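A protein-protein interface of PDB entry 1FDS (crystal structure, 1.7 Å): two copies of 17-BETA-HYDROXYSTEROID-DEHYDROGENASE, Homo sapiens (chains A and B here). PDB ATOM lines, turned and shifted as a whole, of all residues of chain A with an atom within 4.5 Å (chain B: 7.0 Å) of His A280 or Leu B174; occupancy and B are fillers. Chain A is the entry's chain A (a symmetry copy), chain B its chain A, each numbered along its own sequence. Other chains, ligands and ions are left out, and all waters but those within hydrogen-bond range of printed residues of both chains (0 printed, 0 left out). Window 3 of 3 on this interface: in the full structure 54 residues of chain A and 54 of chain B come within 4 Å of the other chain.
No position is printed for both chains.
Of the 6 pairs that touch across the chains among the printed residues, none has its exchanged pair printed and touching as well.
The backbone carbonyl oxygen (O) of Val B171 is in hydrogen-bond range of a ring nitrogen (ND1) of His A280 (2.9 Å).
Among the printed residues, pairs that only touch across the chains: His A280 with Pro B175 (3.3 Å), His A280 with Leu B174 (3.6 Å), Val A276 with Ala B170 (3.8 Å), Val A287 with Pro B175 (3.9 Å) and Met A279 with Val B171 (3.98 Å).
Of chain B, only Val B171 (2.9 Å), Leu B174 (3.6 Å) and Pro B175 (3.3 Å) come within 4 Å of His A280.
Printed residues of chain A within 4 Å of Leu B174: His A280 (3.6 Å).
Printed residues of chain A within 4 Å of Ala B170: Val A276.
Printed residues of chain B within 4 Å of Val A287: Pro B175.
Of the printed residues of chain B, Val A276 touches Ala B170 (3.8 Å).
Printed residues of chain B within 4 Å of Met A279: Val B171 (3.98 Å).
Of the printed residues of chain A, Pro B175 touches His A280 and Val A287.
Val A283 touches none of the printed residues of chain B.
Leu B172 touches none of the printed residues of chain A.
The nearest printed residue of chain A that does not touch Ala B170 is His A280 (5.8 Å).
Printed residues of chain A that touch a printed residue of chain B: Val A276, Met A279, His A280 and Val A287.
Hydrophobic or aromatic side chains of chain A that line the printed part of chain B: Val A276, Met A279, His A280 and Val A287.
Of the 12 printed residues of chain B, 4 touch a printed residue of chain A.
Hydrophobic or aromatic side chains of chain B within 4 Å of the printed part of chain A: Val B171, Leu B174 and Pro B175.
The backbone NH (N) of Gly A285 lies within hydrogen-bond range of the backbone carbonyl oxygen (O) of His A280 (3.3 Å).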
ATOM      1  N   VAL A 276      27.935  10.168 -18.311  1.00  0.00           N
ATOM      2  CA  VAL A 276      27.562  10.352 -19.700  1.00  0.00           C
ATOM      3  C   VAL A 276      26.099  10.736 -19.831  1.00  0.00           C
ATOM      4  O   VAL A 276      25.743  11.642 -20.587  1.00  0.00           O
ATOM      5  CB  VAL A 276      27.867   9.064 -20.514  1.00  0.00           C
ATOM      6  CG1 VAL A 276      27.285   9.133 -21.909  1.00  0.00           C
ATOM      7  CG2 VAL A 276      29.355   8.865 -20.588  1.00  0.00           C
ATOM      8  N   THR A 277      25.247  10.028 -19.101  1.00  0.00           N
ATOM      9  CA  THR A 277      23.815  10.303 -19.123  1.00  0.00           C
ATOM     10  C   THR A 277      23.481  11.691 -18.540  1.00  0.00           C
ATOM     11  O   THR A 277      22.753  12.469 -19.157  1.00  0.00           O
ATOM     12  CB  THR A 277      23.053   9.165 -18.381  1.00  0.00           C
ATOM     13  OG1 THR A 277      23.141   7.963 -19.162  1.00  0.00           O
ATOM     14  CG2 THR A 277      21.599   9.530 -18.168  1.00  0.00           C
ATOM     15  N   ALA A 278      24.058  12.011 -17.388  1.00  0.00           N
ATOM     16  CA  ALA A 278      23.836  13.298 -16.729  1.00  0.00           C
ATOM     17  C   ALA A 278      24.297  14.450 -17.620  1.00  0.00           C
ATOM     18  O   ALA A 278      23.596  15.450 -17.779  1.00  0.00           O
ATOM     19  CB  ALA A 278      24.583  13.341 -15.416  1.00  0.00           C
ATOM     20  N   MET A 279      25.477  14.303 -18.211  1.00  0.00           N
ATOM     21  CA  MET A 279      26.014  15.352 -19.065  1.00  0.00           C
ATOM     22  C   MET A 279      25.199  15.485 -20.341  1.00  0.00           C
ATOM     23  O   MET A 279      24.955  16.592 -20.824  1.00  0.00           O
ATOM     24  CB  MET A 279      27.485  15.088 -19.362  1.00  0.00           C
ATOM     25  CG  MET A 279      28.177  16.256 -20.002  1.00  0.00           C
ATOM     26  SD  MET A 279      28.041  17.751 -18.975  1.00  0.00           S
ATOM     27  CE  MET A 279      28.530  18.893 -20.136  1.00  0.00           C
ATOM     28  N   HIS A 280      24.738  14.366 -20.876  1.00  0.00           N
ATOM     29  CA  HIS A 280      23.935  14.426 -22.076  1.00  0.00           C
ATOM     30  C   HIS A 280      22.618  15.184 -21.813  1.00  0.00           C
ATOM     31  O   HIS A 280      22.214  16.039 -22.614  1.00  0.00           O
ATOM     32  CB  HIS A 280      23.600  13.052 -22.597  1.00  0.00           C
ATOM     33  CG  HIS A 280      22.788  13.097 -23.842  1.00  0.00           C
ATOM     34  ND1 HIS A 280      23.355  13.208 -25.091  1.00  0.00           N
ATOM     35  CD2 HIS A 280      21.448  13.147 -24.030  1.00  0.00           C
ATOM     36  CE1 HIS A 280      22.403  13.335 -25.997  1.00  0.00           C
ATOM     37  NE2 HIS A 280      21.237  13.302 -25.378  1.00  0.00           N
ATOM     38  N   ARG A 281      21.934  14.864 -20.721  1.00  0.00           N
ATOM     39  CA  ARG A 281      20.691  15.571 -20.427  1.00  0.00           C
ATOM     40  C   ARG A 281      20.985  17.046 -20.111  1.00  0.00           C
ATOM     41  O   ARG A 281      20.237  17.931 -20.514  1.00  0.00           O
ATOM     42  CB  ARG A 281      19.940  14.909 -19.266  1.00  0.00           C
ATOM     43  CG  ARG A 281      20.453  15.297 -17.886  1.00  0.00           C
ATOM     44  CD  ARG A 281      19.509  14.851 -16.782  1.00  0.00           C
ATOM     45  NE  ARG A 281      19.958  15.300 -15.464  1.00  0.00           N
ATOM     46  CZ  ARG A 281      19.998  16.572 -15.071  1.00  0.00           C
ATOM     47  NH1 ARG A 281      19.614  17.544 -15.888  1.00  0.00           N
ATOM     48  NH2 ARG A 281      20.420  16.873 -13.850  1.00  0.00           N
ATOM     49  N   GLU A 282      22.095  17.307 -19.430  1.00  0.00           N
ATOM     50  CA  GLU A 282      22.489  18.658 -19.055  1.00  0.00           C
ATOM     51  C   GLU A 282      22.707  19.586 -20.256  1.00  0.00           C
ATOM     52  O   GLU A 282      22.293  20.749 -20.235  1.00  0.00           O
ATOM     53  CB  GLU A 282      23.757  18.603 -18.211  1.00  0.00           C
ATOM     54  CG  GLU A 282      24.222  19.946 -17.674  1.00  0.00           C
ATOM     55  CD  GLU A 282      23.175  20.604 -16.798  1.00  0.00           C
ATOM     56  OE1 GLU A 282      22.609  19.915 -15.912  1.00  0.00           O
ATOM     57  OE2 GLU A 282      22.913  21.810 -17.006  1.00  0.00           O
ATOM     58  N   VAL A 283      23.364  19.070 -21.294  1.00  0.00           N
ATOM     59  CA  VAL A 283      23.652  19.844 -22.506  1.00  0.00           C
ATOM     60  C   VAL A 283      22.560  19.830 -23.594  1.00  0.00           C
ATOM     61  O   VAL A 283      22.279  20.862 -24.210  1.00  0.00           O
ATOM     62  CB  VAL A 283      24.995  19.388 -23.151  1.00  0.00           C
ATOM     63  CG1 VAL A 283      25.348  20.274 -24.343  1.00  0.00           C
ATOM     64  CG2 VAL A 283      26.085  19.411 -22.136  1.00  0.00           C
ATOM     65  N   PHE A 284      21.968  18.666 -23.843  1.00  0.00           N
ATOM     66  CA  PHE A 284      20.970  18.526 -24.883  1.00  0.00           C
ATOM     67  C   PHE A 284      19.561  18.374 -24.316  1.00  0.00           C
ATOM     68  O   PHE A 284      18.704  19.210 -24.549  1.00  0.00           O
ATOM     69  CB  PHE A 284      21.314  17.324 -25.778  1.00  0.00           C
ATOM     70  CG  PHE A 284      22.715  17.357 -26.327  1.00  0.00           C
ATOM     71  CD1 PHE A 284      23.074  18.297 -27.294  1.00  0.00           C
ATOM     72  CD2 PHE A 284      23.695  16.483 -25.842  1.00  0.00           C
ATOM     73  CE1 PHE A 284      24.380  18.373 -27.761  1.00  0.00           C
ATOM     74  CE2 PHE A 284      25.017  16.548 -26.308  1.00  0.00           C
ATOM     75  CZ  PHE A 284      25.358  17.495 -27.265  1.00  0.00           C
ATOM     76  N   GLY A 285      19.341  17.307 -23.563  1.00  0.00           N
ATOM     77  CA  GLY A 285      18.037  17.020 -22.993  1.00  0.00           C
ATOM     78  C   GLY A 285      17.909  15.511 -22.837  1.00  0.00           C
ATOM     79  O   GLY A 285      18.902  14.813 -22.584  1.00  0.00           O
ATOM     80  N   VAL A 287      17.412  11.648 -24.170  1.00  0.00           N
ATOM     81  CA  VAL A 287      17.567  10.736 -25.318  1.00  0.00           C
ATOM     82  C   VAL A 287      17.585   9.280 -24.858  1.00  0.00           C
ATOM     83  O   VAL A 287      17.151   8.966 -23.751  1.00  0.00           O
ATOM     84  CB  VAL A 287      18.847  11.057 -26.094  1.00  0.00           C
ATOM     85  N   LEU B 169      33.277  12.256 -26.694  1.00  0.00           N
ATOM     86  CA  LEU B 169      32.528  11.660 -27.780  1.00  0.00           C
ATOM     87  C   LEU B 169      31.326  10.894 -27.290  1.00  0.00           C
ATOM     88  O   LEU B 169      30.262  11.000 -27.881  1.00  0.00           O
ATOM     89  CB  LEU B 169      33.408  10.730 -28.608  1.00  0.00           C
ATOM     90  CG  LEU B 169      34.293  11.365 -29.672  1.00  0.00           C
ATOM     91  CD1 LEU B 169      35.314  10.335 -30.154  1.00  0.00           C
ATOM     92  CD2 LEU B 169      33.438  11.853 -30.833  1.00  0.00           C
ATOM     93  N   ALA B 170      31.466  10.140 -26.206  1.00  0.00           N
ATOM     94  CA  ALA B 170      30.359   9.349 -25.691  1.00  0.00           C
ATOM     95  C   ALA B 170      29.136  10.189 -25.343  1.00  0.00           C
ATOM     96  O   ALA B 170      28.008   9.741 -25.546  1.00  0.00           O
ATOM     97  CB  ALA B 170      30.799   8.519 -24.489  1.00  0.00           C
ATOM     98  N   VAL B 171      29.346  11.376 -24.784  1.00  0.00           N
ATOM     99  CA  VAL B 171      28.228  12.267 -24.430  1.00  0.00           C
ATOM    100  C   VAL B 171      27.417  12.626 -25.703  1.00  0.00           C
ATOM    101  O   VAL B 171      26.176  12.626 -25.706  1.00  0.00           O
ATOM    102  CB  VAL B 171      28.749  13.543 -23.738  1.00  0.00           C
ATOM    103  CG1 VAL B 171      27.621  14.561 -23.565  1.00  0.00           C
ATOM    104  CG2 VAL B 171      29.363  13.183 -22.360  1.00  0.00           C
ATOM    105  N   LEU B 172      28.116  12.899 -26.792  1.00  0.00           N
ATOM    106  CA  LEU B 172      27.459  13.238 -28.040  1.00  0.00           C
ATOM    107  C   LEU B 172      26.798  12.026 -28.720  1.00  0.00           C
ATOM    108  O   LEU B 172      25.666  12.128 -29.216  1.00  0.00           O
ATOM    109  CB  LEU B 172      28.475  13.870 -29.003  1.00  0.00           C
ATOM    110  CG  LEU B 172      27.981  14.102 -30.441  1.00  0.00           C
ATOM    111  CD1 LEU B 172      26.786  15.066 -30.466  1.00  0.00           C
ATOM    112  CD2 LEU B 172      29.114  14.625 -31.277  1.00  0.00           C
ATOM    113  N   LEU B 173      27.506  10.889 -28.737  1.00  0.00           N
ATOM    114  CA  LEU B 173      27.056   9.670 -29.414  1.00  0.00           C
ATOM    115  C   LEU B 173      25.844   8.948 -28.860  1.00  0.00           C
ATOM    116  O   LEU B 173      25.242   8.156 -29.560  1.00  0.00           O
ATOM    117  CB  LEU B 173      28.210   8.677 -29.522  1.00  0.00           C
ATOM    118  CG  LEU B 173      29.372   9.132 -30.397  1.00  0.00           C
ATOM    119  CD1 LEU B 173      30.439   8.050 -30.377  1.00  0.00           C
ATOM    120  CD2 LEU B 173      28.895   9.396 -31.807  1.00  0.00           C
ATOM    121  N   LEU B 174      25.479   9.228 -27.619  1.00  0.00           N
ATOM    122  CA  LEU B 174      24.356   8.571 -26.976  1.00  0.00           C
ATOM    123  C   LEU B 174      23.143   8.426 -27.903  1.00  0.00           C
ATOM    124  O   LEU B 174      22.703   7.305 -28.169  1.00  0.00           O
ATOM    125  CB  LEU B 174      24.002   9.323 -25.692  1.00  0.00           C
ATOM    126  CG  LEU B 174      23.278   8.603 -24.564  1.00  0.00           C
ATOM    127  CD1 LEU B 174      23.988   7.299 -24.254  1.00  0.00           C
ATOM    128  CD2 LEU B 174      23.264   9.497 -23.333  1.00  0.00           C
ATOM    129  N   PRO B 175      22.638   9.541 -28.481  1.00  0.00           N
ATOM    130  CA  PRO B 175      21.472   9.405 -29.372  1.00  0.00           C
ATOM    131  C   PRO B 175      21.708   8.820 -30.781  1.00  0.00           C
ATOM    132  O   PRO B 175      20.751   8.501 -31.478  1.00  0.00           O
ATOM    133  CB  PRO B 175      20.926  10.835 -29.430  1.00  0.00           C
ATOM    134  CG  PRO B 175      22.174  11.668 -29.328  1.00  0.00           C
ATOM    135  CD  PRO B 175      22.947  10.962 -28.239  1.00  0.00           C
ATOM    136  N   PHE B 176      22.957   8.636 -31.193  1.00  0.00           N
ATOM    137  CA  PHE B 176      23.233   8.095 -32.514  1.00  0.00           C
ATOM    138  C   PHE B 176      23.226   6.573 -32.596  1.00  0.00           C
ATOM    139  O   PHE B 176      23.296   6.006 -33.683  1.00  0.00           O
ATOM    140  CB  PHE B 176      24.559   8.606 -33.023  1.00  0.00           C
ATOM    141  CG  PHE B 176      24.561  10.060 -33.314  1.00  0.00           C
ATOM    142  CD1 PHE B 176      24.681  10.990 -32.289  1.00  0.00           C
ATOM    143  CD2 PHE B 176      24.456  10.506 -34.619  1.00  0.00           C
ATOM    144  CE1 PHE B 176      24.701  12.354 -32.559  1.00  0.00           C
ATOM    145  CE2 PHE B 176      24.475  11.867 -34.904  1.00  0.00           C
ATOM    146  CZ  PHE B 176      24.600  12.789 -33.870  1.00  0.00           C
ATOM    147  N   GLY B 177      23.169   5.907 -31.455  1.00  0.00           N
ATOM    148  CA  GLY B 177      23.181   4.457 -31.495  1.00  0.00           C
ATOM    149  C   GLY B 177      24.574   3.898 -31.746  1.00  0.00           C
ATOM    150  O   GLY B 177      24.701   2.711 -32.060  1.00  0.00           O
ATOM    151  N   VAL B 178      25.606   4.740 -31.641  1.00  0.00           N
ATOM    152  CA  VAL B 178      27.003   4.315 -31.830  1.00  0.00           C
ATOM    153  C   VAL B 178      27.569   4.220 -30.421  1.00  0.00           C
ATOM    154  O   VAL B 178      27.483   5.166 -29.645  1.00  0.00           O
ATOM    155  CB  VAL B 178      27.824   5.332 -32.669  1.00  0.00           C
ATOM    156  CG1 VAL B 178      29.287   4.843 -32.839  1.00  0.00           C
ATOM    157  CG2 VAL B 178      27.158   5.543 -34.054  1.00  0.00           C
ATOM    158  N   HIS B 179      28.104   3.055 -30.070  1.00  0.00           N
ATOM    159  CA  HIS B 179      28.629   2.833 -28.728  1.00  0.00           C
ATOM    160  C   HIS B 179      30.127   2.875 -28.661  1.00  0.00           C
ATOM    161  O   HIS B 179      30.789   2.287 -29.499  1.00  0.00           O
ATOM    162  CB  HIS B 179      28.148   1.495 -28.230  1.00  0.00           C
ATOM    163  CG  HIS B 179      26.672   1.428 -28.131  1.00  0.00           C
ATOM    164  ND1 HIS B 179      25.897   0.770 -29.059  1.00  0.00           N
ATOM    165  CD2 HIS B 179      25.818   1.988 -27.245  1.00  0.00           C
ATOM    166  CE1 HIS B 179      24.624   0.926 -28.750  1.00  0.00           C
ATOM    167  NE2 HIS B 179      24.551   1.661 -27.653  1.00  0.00           N
ATOM    168  N   LYS B 248      23.749  -2.769 -24.097  1.00  0.00           N
ATOM    169  CA  LYS B 248      23.896  -1.353 -23.766  1.00  0.00           C
ATOM    170  C   LYS B 248      25.247  -1.222 -23.056  1.00  0.00           C
ATOM    171  O   LYS B 248      25.333  -1.181 -21.818  1.00  0.00           O
ATOM    172  CB  LYS B 248      22.739  -0.940 -22.855  1.00  0.00           C
ATOM    173  CG  LYS B 248      22.697   0.520 -22.458  1.00  0.00           C
ATOM    174  CD  LYS B 248      22.658   1.465 -23.647  1.00  0.00           C
ATOM    175  CE  LYS B 248      22.175   2.848 -23.197  1.00  0.00           C
ATOM    176  NZ  LYS B 248      22.787   3.310 -21.898  1.00  0.00           N
